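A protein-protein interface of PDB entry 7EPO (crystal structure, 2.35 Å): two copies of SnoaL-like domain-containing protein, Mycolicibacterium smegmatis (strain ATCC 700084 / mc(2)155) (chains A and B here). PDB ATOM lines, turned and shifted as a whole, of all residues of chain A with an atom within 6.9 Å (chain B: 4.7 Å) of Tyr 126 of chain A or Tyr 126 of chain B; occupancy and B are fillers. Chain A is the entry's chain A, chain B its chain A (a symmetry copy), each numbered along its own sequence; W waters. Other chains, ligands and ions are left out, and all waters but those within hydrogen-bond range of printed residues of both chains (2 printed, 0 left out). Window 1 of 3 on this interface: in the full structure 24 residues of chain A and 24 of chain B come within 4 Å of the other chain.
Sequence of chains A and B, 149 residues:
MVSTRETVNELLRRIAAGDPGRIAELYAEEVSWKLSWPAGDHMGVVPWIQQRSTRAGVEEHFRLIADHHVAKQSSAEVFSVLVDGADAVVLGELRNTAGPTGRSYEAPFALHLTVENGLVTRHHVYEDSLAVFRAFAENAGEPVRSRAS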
ATOM      1  N   LYS A  34       4.868  -7.861  37.075  1.00  0.00           N
ATOM      2  CA  LYS A  34       3.664  -7.410  36.389  1.00  0.00           C
ATOM      3  C   LYS A  34       3.313  -8.334  35.235  1.00  0.00           C
ATOM      4  O   LYS A  34       4.177  -8.980  34.629  1.00  0.00           O
ATOM      5  CB  LYS A  34       3.792  -5.981  35.850  1.00  0.00           C
ATOM      6  CG  LYS A  34       4.181  -4.962  36.875  1.00  0.00           C
ATOM      7  CD  LYS A  34       3.958  -3.544  36.382  1.00  0.00           C
ATOM      8  CE  LYS A  34       4.303  -2.530  37.486  1.00  0.00           C
ATOM      9  NZ  LYS A  34       4.515  -1.182  36.911  1.00  0.00           N
ATOM     10  N   LEU A  35       2.021  -8.368  34.932  1.00  0.00           N
ATOM     11  CA  LEU A  35       1.482  -9.239  33.907  1.00  0.00           C
ATOM     12  C   LEU A  35       0.382  -8.501  33.156  1.00  0.00           C
ATOM     13  O   LEU A  35      -0.415  -7.786  33.772  1.00  0.00           O
ATOM     14  CB  LEU A  35       0.940 -10.531  34.527  1.00  0.00           C
ATOM     15  CG  LEU A  35       1.836 -11.270  35.530  1.00  0.00           C
ATOM     16  CD1 LEU A  35       1.077 -12.386  36.239  1.00  0.00           C
ATOM     17  CD2 LEU A  35       3.090 -11.835  34.842  1.00  0.00           C
ATOM     18  N   SER A  36       0.334  -8.683  31.830  1.00  0.00           N
ATOM     19  CA  SER A  36      -0.717  -8.091  30.999  1.00  0.00           C
ATOM     20  C   SER A  36      -1.988  -8.952  31.039  1.00  0.00           C
ATOM     21  O   SER A  36      -2.444  -9.520  30.043  1.00  0.00           O
ATOM     22  CB  SER A  36      -0.229  -7.888  29.568  1.00  0.00           C
ATOM     23  OG  SER A  36       0.124  -9.117  28.959  1.00  0.00           O
ATOM     24  N   PHE A  79      12.637 -15.531  20.005  1.00  0.00           N
ATOM     25  CA  PHE A  79      12.973 -14.924  18.730  1.00  0.00           C
ATOM     26  C   PHE A  79      14.154 -13.965  18.848  1.00  0.00           C
ATOM     27  O   PHE A  79      15.040 -13.974  17.985  1.00  0.00           O
ATOM     28  CB  PHE A  79      11.741 -14.221  18.163  1.00  0.00           C
ATOM     29  CG  PHE A  79      10.613 -15.147  17.868  1.00  0.00           C
ATOM     30  CD1 PHE A  79      10.803 -16.266  17.069  1.00  0.00           C
ATOM     31  CD2 PHE A  79       9.348 -14.913  18.405  1.00  0.00           C
ATOM     32  CE1 PHE A  79       9.746 -17.133  16.792  1.00  0.00           C
ATOM     33  CE2 PHE A  79       8.291 -15.770  18.141  1.00  0.00           C
ATOM     34  CZ  PHE A  79       8.485 -16.884  17.330  1.00  0.00           C
ATOM     35  N   VAL A  89      14.227  -6.890  26.819  1.00  0.00           N
ATOM     36  CA  VAL A  89      12.951  -7.454  26.413  1.00  0.00           C
ATOM     37  C   VAL A  89      13.206  -8.760  25.673  1.00  0.00           C
ATOM     38  O   VAL A  89      13.834  -8.763  24.610  1.00  0.00           O
ATOM     39  CB  VAL A  89      12.136  -6.495  25.536  1.00  0.00           C
ATOM     40  CG1 VAL A  89      10.887  -7.222  25.039  1.00  0.00           C
ATOM     41  CG2 VAL A  89      11.770  -5.250  26.322  1.00  0.00           C
ATOM     42  N   VAL A  90      12.691  -9.858  26.215  1.00  0.00           N
ATOM     43  CA  VAL A  90      12.747 -11.148  25.551  1.00  0.00           C
ATOM     44  C   VAL A  90      11.486 -11.318  24.722  1.00  0.00           C
ATOM     45  O   VAL A  90      10.367 -11.252  25.250  1.00  0.00           O
ATOM     46  CB  VAL A  90      12.887 -12.282  26.568  1.00  0.00           C
ATOM     47  CG1 VAL A  90      13.263 -13.572  25.857  1.00  0.00           C
ATOM     48  CG2 VAL A  90      13.912 -11.887  27.606  1.00  0.00           C
ATOM     49  N   LEU A  91      11.675 -11.542  23.424  1.00  0.00           N
ATOM     50  CA  LEU A  91      10.598 -11.701  22.459  1.00  0.00           C
ATOM     51  C   LEU A  91      10.556 -13.166  22.052  1.00  0.00           C
ATOM     52  O   LEU A  91      11.552 -13.697  21.545  1.00  0.00           O
ATOM     53  CB  LEU A  91      10.847 -10.822  21.236  1.00  0.00           C
ATOM     54  CG  LEU A  91      10.891  -9.309  21.434  1.00  0.00           C
ATOM     55  CD1 LEU A  91      11.340  -8.698  20.121  1.00  0.00           C
ATOM     56  CD2 LEU A  91       9.532  -8.742  21.825  1.00  0.00           C
ATOM     57  N   GLY A  92       9.437 -13.815  22.287  1.00  0.00           N
ATOM     58  CA  GLY A  92       9.292 -15.208  21.902  1.00  0.00           C
ATOM     59  C   GLY A  92       7.833 -15.611  21.847  1.00  0.00           C
ATOM     60  O   GLY A  92       6.955 -14.780  21.722  1.00  0.00           O
ATOM     61  N   GLU A  93       7.611 -16.930  21.955  1.00  0.00           N
ATOM     62  CA  GLU A  93       6.281 -17.515  21.874  1.00  0.00           C
ATOM     63  C   GLU A  93       6.208 -18.710  22.813  1.00  0.00           C
ATOM     64  O   GLU A  93       7.106 -19.551  22.800  1.00  0.00           O
ATOM     65  CB  GLU A  93       5.968 -17.943  20.440  1.00  0.00           C
ATOM     66  CG  GLU A  93       4.500 -18.255  20.160  1.00  0.00           C
ATOM     67  CD  GLU A  93       4.245 -18.526  18.676  1.00  0.00           C
ATOM     68  OE1 GLU A  93       4.881 -19.449  18.116  1.00  0.00           O
ATOM     69  OE2 GLU A  93       3.413 -17.818  18.073  1.00  0.00           O
ATOM     70  N   ALA A 107       0.892 -18.565  22.809  1.00  0.00           N
ATOM     71  CA  ALA A 107       0.819 -17.183  23.270  1.00  0.00           C
ATOM     72  C   ALA A 107       2.120 -16.477  22.927  1.00  0.00           C
ATOM     73  O   ALA A 107       3.178 -16.833  23.482  1.00  0.00           O
ATOM     74  CB  ALA A 107       0.543 -17.116  24.770  1.00  0.00           C
ATOM     75  N   PRO A 108       2.102 -15.505  22.019  1.00  0.00           N
ATOM     76  CA  PRO A 108       3.267 -14.626  21.874  1.00  0.00           C
ATOM     77  C   PRO A 108       3.509 -13.846  23.156  1.00  0.00           C
ATOM     78  O   PRO A 108       2.569 -13.442  23.850  1.00  0.00           O
ATOM     79  CB  PRO A 108       2.873 -13.701  20.718  1.00  0.00           C
ATOM     80  CG  PRO A 108       1.922 -14.539  19.883  1.00  0.00           C
ATOM     81  CD  PRO A 108       1.158 -15.382  20.894  1.00  0.00           C
ATOM     82  N   PHE A 109       4.785 -13.635  23.472  1.00  0.00           N
ATOM     83  CA  PHE A 109       5.123 -12.870  24.657  1.00  0.00           C
ATOM     84  C   PHE A 109       6.281 -11.929  24.373  1.00  0.00           C
ATOM     85  O   PHE A 109       7.148 -12.197  23.538  1.00  0.00           O
ATOM     86  CB  PHE A 109       5.483 -13.767  25.854  1.00  0.00           C
ATOM     87  CG  PHE A 109       6.816 -14.457  25.715  1.00  0.00           C
ATOM     88  CD1 PHE A 109       7.987 -13.837  26.123  1.00  0.00           C
ATOM     89  CD2 PHE A 109       6.892 -15.734  25.177  1.00  0.00           C
ATOM     90  CE1 PHE A 109       9.210 -14.465  25.981  1.00  0.00           C
ATOM     91  CE2 PHE A 109       8.116 -16.380  25.049  1.00  0.00           C
ATOM     92  CZ  PHE A 109       9.277 -15.733  25.449  1.00  0.00           C
ATOM     93  N   ALA A 110       6.267 -10.822  25.098  1.00  0.00           N
ATOM     94  CA  ALA A 110       7.404  -9.940  25.262  1.00  0.00           C
ATOM     95  C   ALA A 110       7.668  -9.862  26.759  1.00  0.00           C
ATOM     96  O   ALA A 110       6.786  -9.448  27.516  1.00  0.00           O
ATOM     97  CB  ALA A 110       7.120  -8.555  24.662  1.00  0.00           C
ATOM     98  N   LEU A 111       8.866 -10.293  27.188  1.00  0.00           N
ATOM     99  CA  LEU A 111       9.238 -10.359  28.604  1.00  0.00           C
ATOM    100  C   LEU A 111      10.194  -9.209  28.897  1.00  0.00           C
ATOM    101  O   LEU A 111      11.329  -9.187  28.401  1.00  0.00           O
ATOM    102  CB  LEU A 111       9.871 -11.709  28.935  1.00  0.00           C
ATOM    103  CG  LEU A 111      10.452 -11.911  30.324  1.00  0.00           C
ATOM    104  CD1 LEU A 111       9.400 -11.691  31.387  1.00  0.00           C
ATOM    105  CD2 LEU A 111      10.976 -13.302  30.446  1.00  0.00           C
ATOM    106  N   HIS A 112       9.729  -8.248  29.679  1.00  0.00           N
ATOM    107  CA  HIS A 112      10.513  -7.066  30.022  1.00  0.00           C
ATOM    108  C   HIS A 112      11.259  -7.333  31.324  1.00  0.00           C
ATOM    109  O   HIS A 112      10.634  -7.654  32.341  1.00  0.00           O
ATOM    110  CB  HIS A 112       9.596  -5.848  30.161  1.00  0.00           C
ATOM    111  CG  HIS A 112      10.280  -4.605  30.651  1.00  0.00           C
ATOM    112  ND1 HIS A 112      11.631  -4.375  30.500  1.00  0.00           N
ATOM    113  CD2 HIS A 112       9.790  -3.534  31.319  1.00  0.00           C
ATOM    114  CE1 HIS A 112      11.938  -3.207  31.038  1.00  0.00           C
ATOM    115  NE2 HIS A 112      10.838  -2.676  31.539  1.00  0.00           N
ATOM    116  N   HIS A 124       8.181  -8.239  33.893  1.00  0.00           N
ATOM    117  CA  HIS A 124       6.884  -7.736  33.434  1.00  0.00           C
ATOM    118  C   HIS A 124       6.549  -8.455  32.133  1.00  0.00           C
ATOM    119  O   HIS A 124       7.182  -8.209  31.100  1.00  0.00           O
ATOM    120  CB  HIS A 124       6.900  -6.219  33.211  1.00  0.00           C
ATOM    121  CG  HIS A 124       7.105  -5.400  34.454  1.00  0.00           C
ATOM    122  ND1 HIS A 124       7.039  -4.022  34.448  1.00  0.00           N
ATOM    123  CD2 HIS A 124       7.376  -5.755  35.735  1.00  0.00           C
ATOM    124  CE1 HIS A 124       7.250  -3.564  35.669  1.00  0.00           C
ATOM    125  NE2 HIS A 124       7.458  -4.596  36.467  1.00  0.00           N
ATOM    126  N   VAL A 125       5.575  -9.341  32.178  1.00  0.00           N
ATOM    127  CA  VAL A 125       5.210 -10.132  31.010  1.00  0.00           C
ATOM    128  C   VAL A 125       4.124  -9.400  30.243  1.00  0.00           C
ATOM    129  O   VAL A 125       3.132  -8.950  30.834  1.00  0.00           O
ATOM    130  CB  VAL A 125       4.735 -11.532  31.426  1.00  0.00           C
ATOM    131  CG1 VAL A 125       4.126 -12.268  30.231  1.00  0.00           C
ATOM    132  CG2 VAL A 125       5.876 -12.315  32.043  1.00  0.00           C
ATOM    133  N   TYR A 126       4.296  -9.311  28.921  1.00  0.00           N
ATOM    134  CA  TYR A 126       3.265  -8.862  27.987  1.00  0.00           C
ATOM    135  C   TYR A 126       2.975 -10.020  27.043  1.00  0.00           C
ATOM    136  O   TYR A 126       3.868 -10.452  26.303  1.00  0.00           O
ATOM    137  CB  TYR A 126       3.733  -7.637  27.209  1.00  0.00           C
ATOM    138  CG  TYR A 126       4.010  -6.437  28.089  1.00  0.00           C
ATOM    139  CD1 TYR A 126       5.200  -6.331  28.767  1.00  0.00           C
ATOM    140  CD2 TYR A 126       3.075  -5.418  28.228  1.00  0.00           C
ATOM    141  CE1 TYR A 126       5.475  -5.247  29.566  1.00  0.00           C
ATOM    142  CE2 TYR A 126       3.331  -4.325  29.018  1.00  0.00           C
ATOM    143  CZ  TYR A 126       4.545  -4.240  29.681  1.00  0.00           C
ATOM    144  OH  TYR A 126       4.834  -3.160  30.475  1.00  0.00           O
ATOM    145  N   GLU A 127       1.742 -10.532  27.064  1.00  0.00           N
ATOM    146  CA  GLU A 127       1.446 -11.762  26.332  1.00  0.00           C
ATOM    147  C   GLU A 127      -0.033 -11.871  25.972  1.00  0.00           C
ATOM    148  O   GLU A 127      -0.891 -11.208  26.562  1.00  0.00           O
ATOM    149  CB  GLU A 127       1.846 -12.993  27.137  1.00  0.00           C
ATOM    150  CG  GLU A 127       0.772 -13.449  28.112  1.00  0.00           C
ATOM    151  CD  GLU A 127       1.324 -14.344  29.207  1.00  0.00           C
ATOM    152  OE1 GLU A 127       2.305 -15.079  28.934  1.00  0.00           O
ATOM    153  OE2 GLU A 127       0.791 -14.296  30.339  1.00  0.00           O
ATOM    154  N   ASP A 128      -0.317 -12.747  24.994  1.00  0.00           N
ATOM    155  CA  ASP A 128      -1.673 -12.983  24.492  1.00  0.00           C
ATOM    156  C   ASP A 128      -2.503 -13.624  25.598  1.00  0.00           C
ATOM    157  O   ASP A 128      -2.685 -14.839  25.669  1.00  0.00           O
ATOM    158  CB  ASP A 128      -1.664 -13.853  23.243  1.00  0.00           C
ATOM    159  CG  ASP A 128      -3.043 -13.948  22.590  1.00  0.00           C
ATOM    160  OD1 ASP A 128      -4.036 -13.510  23.210  1.00  0.00           O
ATOM    161  OD2 ASP A 128      -3.146 -14.459  21.457  1.00  0.00           O
ATOM    162  N   SER A 129      -3.024 -12.764  26.469  1.00  0.00           N
ATOM    163  CA  SER A 129      -3.743 -13.217  27.652  1.00  0.00           C
ATOM    164  C   SER A 129      -5.027 -13.947  27.271  1.00  0.00           C
ATOM    165  O   SER A 129      -5.387 -14.949  27.902  1.00  0.00           O
ATOM    166  CB  SER A 129      -4.036 -12.020  28.562  1.00  0.00           C
ATOM    167  OG  SER A 129      -4.726 -10.982  27.879  1.00  0.00           O
ATOM    168  N   SER B  36      -0.566  -9.889  19.555  1.00  0.00           N
ATOM    169  CA  SER B  36      -0.738 -10.973  20.524  1.00  0.00           C
ATOM    170  C   SER B  36      -2.229 -11.225  20.795  1.00  0.00           C
ATOM    171  O   SER B  36      -2.747 -11.050  21.901  1.00  0.00           O
ATOM    172  CB  SER B  36       0.019 -10.673  21.814  1.00  0.00           C
ATOM    173  OG  SER B  36      -0.460  -9.495  22.437  1.00  0.00           O
ATOM    174  N   LEU B  91       7.045   0.612  25.821  1.00  0.00           N
ATOM    175  CA  LEU B  91       6.366   0.063  26.985  1.00  0.00           C
ATOM    176  C   LEU B  91       5.410   1.125  27.505  1.00  0.00           C
ATOM    177  O   LEU B  91       5.842   2.233  27.850  1.00  0.00           O
ATOM    178  CB  LEU B  91       7.378  -0.306  28.065  1.00  0.00           C
ATOM    179  CG  LEU B  91       8.410  -1.387  27.746  1.00  0.00           C
ATOM    180  CD1 LEU B  91       9.396  -1.418  28.896  1.00  0.00           C
ATOM    181  CD2 LEU B  91       7.769  -2.759  27.580  1.00  0.00           C
ATOM    182  N   GLY B  92       4.134   0.809  27.539  1.00  0.00           N
ATOM    183  CA  GLY B  92       3.150   1.747  28.052  1.00  0.00           C
ATOM    184  C   GLY B  92       1.861   1.042  28.417  1.00  0.00           C
ATOM    185  O   GLY B  92       1.839  -0.152  28.644  1.00  0.00           O
ATOM    186  N   PRO B 108      -2.121  -2.980  29.342  1.00  0.00           N
ATOM    187  CA  PRO B 108      -0.672  -2.806  29.191  1.00  0.00           C
ATOM    188  C   PRO B 108      -0.214  -3.302  27.830  1.00  0.00           C
ATOM    189  O   PRO B 108      -0.730  -4.293  27.301  1.00  0.00           O
ATOM    190  CB  PRO B 108      -0.093  -3.655  30.327  1.00  0.00           C
ATOM    191  CG  PRO B 108      -1.174  -3.637  31.392  1.00  0.00           C
ATOM    192  CD  PRO B 108      -2.482  -3.630  30.614  1.00  0.00           C
ATOM    193  N   PHE B 109       0.765  -2.605  27.260  1.00  0.00           N
ATOM    194  CA  PHE B 109       1.300  -3.018  25.976  1.00  0.00           C
ATOM    195  C   PHE B 109       2.813  -2.882  25.959  1.00  0.00           C
ATOM    196  O   PHE B 109       3.397  -2.028  26.630  1.00  0.00           O
ATOM    197  CB  PHE B 109       0.707  -2.215  24.806  1.00  0.00           C
ATOM    198  CG  PHE B 109       1.195  -0.790  24.739  1.00  0.00           C
ATOM    199  CD1 PHE B 109       2.365  -0.467  24.067  1.00  0.00           C
ATOM    200  CD2 PHE B 109       0.476   0.228  25.350  1.00  0.00           C
ATOM    201  CE1 PHE B 109       2.819   0.838  24.020  1.00  0.00           C
ATOM    202  CE2 PHE B 109       0.917   1.544  25.290  1.00  0.00           C
ATOM    203  CZ  PHE B 109       2.098   1.843  24.625  1.00  0.00           C
ATOM    204  N   ALA B 110       3.423  -3.749  25.167  1.00  0.00           N
ATOM    205  CA  ALA B 110       4.795  -3.620  24.720  1.00  0.00           C
ATOM    206  C   ALA B 110       4.745  -3.610  23.198  1.00  0.00           C
ATOM    207  O   ALA B 110       4.265  -4.574  22.595  1.00  0.00           O
ATOM    208  CB  ALA B 110       5.660  -4.769  25.254  1.00  0.00           C
ATOM    209  N   HIS B 112       6.739  -3.591  19.820  1.00  0.00           N
ATOM    210  CA  HIS B 112       8.034  -3.935  19.243  1.00  0.00           C
ATOM    211  C   HIS B 112       8.124  -3.330  17.846  1.00  0.00           C
ATOM    212  O   HIS B 112       7.269  -3.606  16.996  1.00  0.00           O
ATOM    213  CB  HIS B 112       8.199  -5.456  19.189  1.00  0.00           C
ATOM    214  CG  HIS B 112       9.437  -5.923  18.481  1.00  0.00           C
ATOM    215  ND1 HIS B 112      10.572  -5.151  18.351  1.00  0.00           N
ATOM    216  CD2 HIS B 112       9.700  -7.086  17.839  1.00  0.00           C
ATOM    217  CE1 HIS B 112      11.485  -5.826  17.676  1.00  0.00           C
ATOM    218  NE2 HIS B 112      10.981  -7.004  17.355  1.00  0.00           N
ATOM    219  N   HIS B 124       4.848  -4.985  15.995  1.00  0.00           N
ATOM    220  CA  HIS B 124       4.372  -6.203  16.654  1.00  0.00           C
ATOM    221  C   HIS B 124       3.893  -5.812  18.047  1.00  0.00           C
ATOM    222  O   HIS B 124       4.705  -5.476  18.916  1.00  0.00           O
ATOM    223  CB  HIS B 124       5.467  -7.273  16.752  1.00  0.00           C
ATOM    224  CG  HIS B 124       5.933  -7.820  15.432  1.00  0.00           C
ATOM    225  ND1 HIS B 124       6.834  -8.863  15.345  1.00  0.00           N
ATOM    226  CD2 HIS B 124       5.634  -7.477  14.155  1.00  0.00           C
ATOM    227  CE1 HIS B 124       7.061  -9.144  14.074  1.00  0.00           C
ATOM    228  NE2 HIS B 124       6.346  -8.317  13.333  1.00  0.00           N
ATOM    229  N   VAL B 125       2.593  -5.844  18.258  1.00  0.00           N
ATOM    230  CA  VAL B 125       2.019  -5.431  19.532  1.00  0.00           C
ATOM    231  C   VAL B 125       1.906  -6.647  20.435  1.00  0.00           C
ATOM    232  O   VAL B 125       1.405  -7.698  20.012  1.00  0.00           O
ATOM    233  CB  VAL B 125       0.645  -4.776  19.325  1.00  0.00           C
ATOM    234  CG1 VAL B 125      -0.058  -4.568  20.668  1.00  0.00           C
ATOM    235  CG2 VAL B 125       0.790  -3.474  18.563  1.00  0.00           C
ATOM    236  N   TYR B 126       2.342  -6.491  21.689  1.00  0.00           N
ATOM    237  CA  TYR B 126       2.106  -7.450  22.766  1.00  0.00           C
ATOM    238  C   TYR B 126       1.289  -6.738  23.834  1.00  0.00           C
ATOM    239  O   TYR B 126       1.762  -5.756  24.420  1.00  0.00           O
ATOM    240  CB  TYR B 126       3.424  -7.955  23.342  1.00  0.00           C
ATOM    241  CG  TYR B 126       4.272  -8.700  22.335  1.00  0.00           C
ATOM    242  CD1 TYR B 126       5.051  -8.014  21.434  1.00  0.00           C
ATOM    243  CD2 TYR B 126       4.290 -10.090  22.299  1.00  0.00           C
ATOM    244  CE1 TYR B 126       5.834  -8.670  20.516  1.00  0.00           C
ATOM    245  CE2 TYR B 126       5.067 -10.766  21.393  1.00  0.00           C
ATOM    246  CZ  TYR B 126       5.849 -10.046  20.503  1.00  0.00           C
ATOM    247  OH  TYR B 126       6.641 -10.690  19.587  1.00  0.00           O
ATOM    248  N   GLU B 127       0.069  -7.216  24.090  1.00  0.00           N
ATOM    249  CA  GLU B 127      -0.842  -6.472  24.959  1.00  0.00           C
ATOM    250  C   GLU B 127      -1.885  -7.380  25.604  1.00  0.00           C
ATOM    251  O   GLU B 127      -2.147  -8.493  25.139  1.00  0.00           O
ATOM    252  CB  GLU B 127      -1.561  -5.370  24.190  1.00  0.00           C
ATOM    253  CG  GLU B 127      -2.814  -5.852  23.478  1.00  0.00           C
ATOM    254  CD  GLU B 127      -3.251  -4.911  22.370  1.00  0.00           C
ATOM    255  OE1 GLU B 127      -3.015  -3.684  22.505  1.00  0.00           O
ATOM    256  OE2 GLU B 127      -3.810  -5.398  21.361  1.00  0.00           O
HETATM  257  O   HOH W   1       3.205  -1.320  30.582  1.00  0.00           O
HETATM  258  O   HOH W   2       6.740 -13.148  19.654  1.00  0.00           O
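O of Glu 127 of chain B sits close to O of Glu 127 of chain A (3.3 Å).
The side-chain carboxylate of Asp 128 of chain A lies close to the backbone carbonyl oxygen of Ser 36 of chain B.
The backbone NH of Glu 127 of chain A lies within hydrogen-bond range of the side-chain hydroxyl of Ser 36 of chain A (2.9 Å).
N of Phe 79 of chain A sits at hydrogen-bond distance from O of Leu 91 of chain A, at 2.6 Å.
The backbone carbonyl oxygen (O) of Gly 92 of chain A sits at hydrogen-bond distance from the backbone NH (N) of Phe 109 of chain A (3.0 Å).
The backbone NH (N) of His 112 of chain A lies within hydrogen-bond range of the backbone carbonyl oxygen (O) of His 124 of chain A, 2.9 Å away.
The backbone NH of Phe 109 of chain B lies within hydrogen-bond range of the backbone carbonyl oxygen of Gly 92 of chain B (3.0 Å).
The backbone carbonyl oxygen of His 124 of chain B is in hydrogen-bond range of the backbone NH of His 112 of chain B (2.9 Å).
Among the printed residues, pairs that only touch across the chains: Leu 91 of chain A with His 112 of chain B, Leu 91 of chain A with Tyr 126 of chain B, Pro 108 of chain A with Tyr 126 of chain B, Phe 109 of chain A with Tyr 126 of chain B, Ala 110 of chain A with Tyr 126 of chain B, His 112 of chain A with Leu 91 of chain B, Tyr 126 of chain A with Leu 91 of chain B, Tyr 126 of chain A with Pro 108 of chain B, Tyr 126 of chain A with Phe 109 of chain B, Tyr 126 of chain A with Ala 110 of chain B and Tyr 126 of chain A with Tyr 126 of chain B.
Of the printed residues of chain B, Leu 91 of chain A touches His 112 (3.2 Å) and Tyr 126 (3.9 Å).
Tyr 126 of chain A touches five residues of chain B.
Printed residues of chain A within 4 Å of Ser 36 of chain B: Asp 128 (3.0 Å).
Of the printed residues of chain A, Phe 109 of chain B touches Tyr 126 (3.3 Å).
Tyr 126 of chain B touches just these residues of chain A: Leu 91, Pro 108, Phe 109, Ala 110 and Tyr 126.
Printed residues of chain A within 4 Å of Glu 127 of chain B: Glu 127 (3.3 Å).
The nearest residue of chain B that does not touch Tyr 126 of chain A is Gly 92 of chain B (4.4 Å).
The nearest printed residue of chain A that does not touch Glu 127 of chain B is Ser 36 of chain A (4.3 Å).
Of the 21 printed residues of chain A, 8 touch a printed residue of chain B.
Printed residues of chain A that touch a printed residue of chain B: Leu 91, Pro 108, Phe 109, Ala 110, His 112, Tyr 126, Glu 127 and Asp 128.
Hydrophobic or aromatic side chains of chain A that line the printed part of chain B: Leu 91, Pro 108, Ala 110, His 112 and Tyr 126.
Hydrophobic or aromatic side chains of chain B within 4 Å of the printed part of chain A: Leu 91, Pro 108, Ala 110, His 112 and Tyr 126.
Among the printed residues, no Asp or Glu carboxylate lies within 4 Å of a Lys or Arg side-chain nitrogen of the other chain.
Leu 91 of chain A touches His 112 of chain B, and with the chains exchanged His 112 of chain A touches Leu 91 of chain B.
Leu 91 of chain A touches Tyr 126 of chain B, and with the chains exchanged Tyr 126 of chain A touches Leu 91 of chain B.
Pro 108 of chain A touches Tyr 126 of chain B, and with the chains exchanged Tyr 126 of chain A touches Pro 108 of chain B.
Ala 110 of chain A touches Tyr 126 of chain B, and with the chains exchanged Tyr 126 of chain A touches Ala 110 of chain B.
Water W1 lies within hydrogen-bond range of OH of Tyr 126 of chain A (2.5 Å) and O of Gly 92 of chain B (2.6 Å).
Water W2 bridges OH of Tyr 126 of chain B (2.5 Å) and O of Gly 92 of chain A (2.6 Å).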
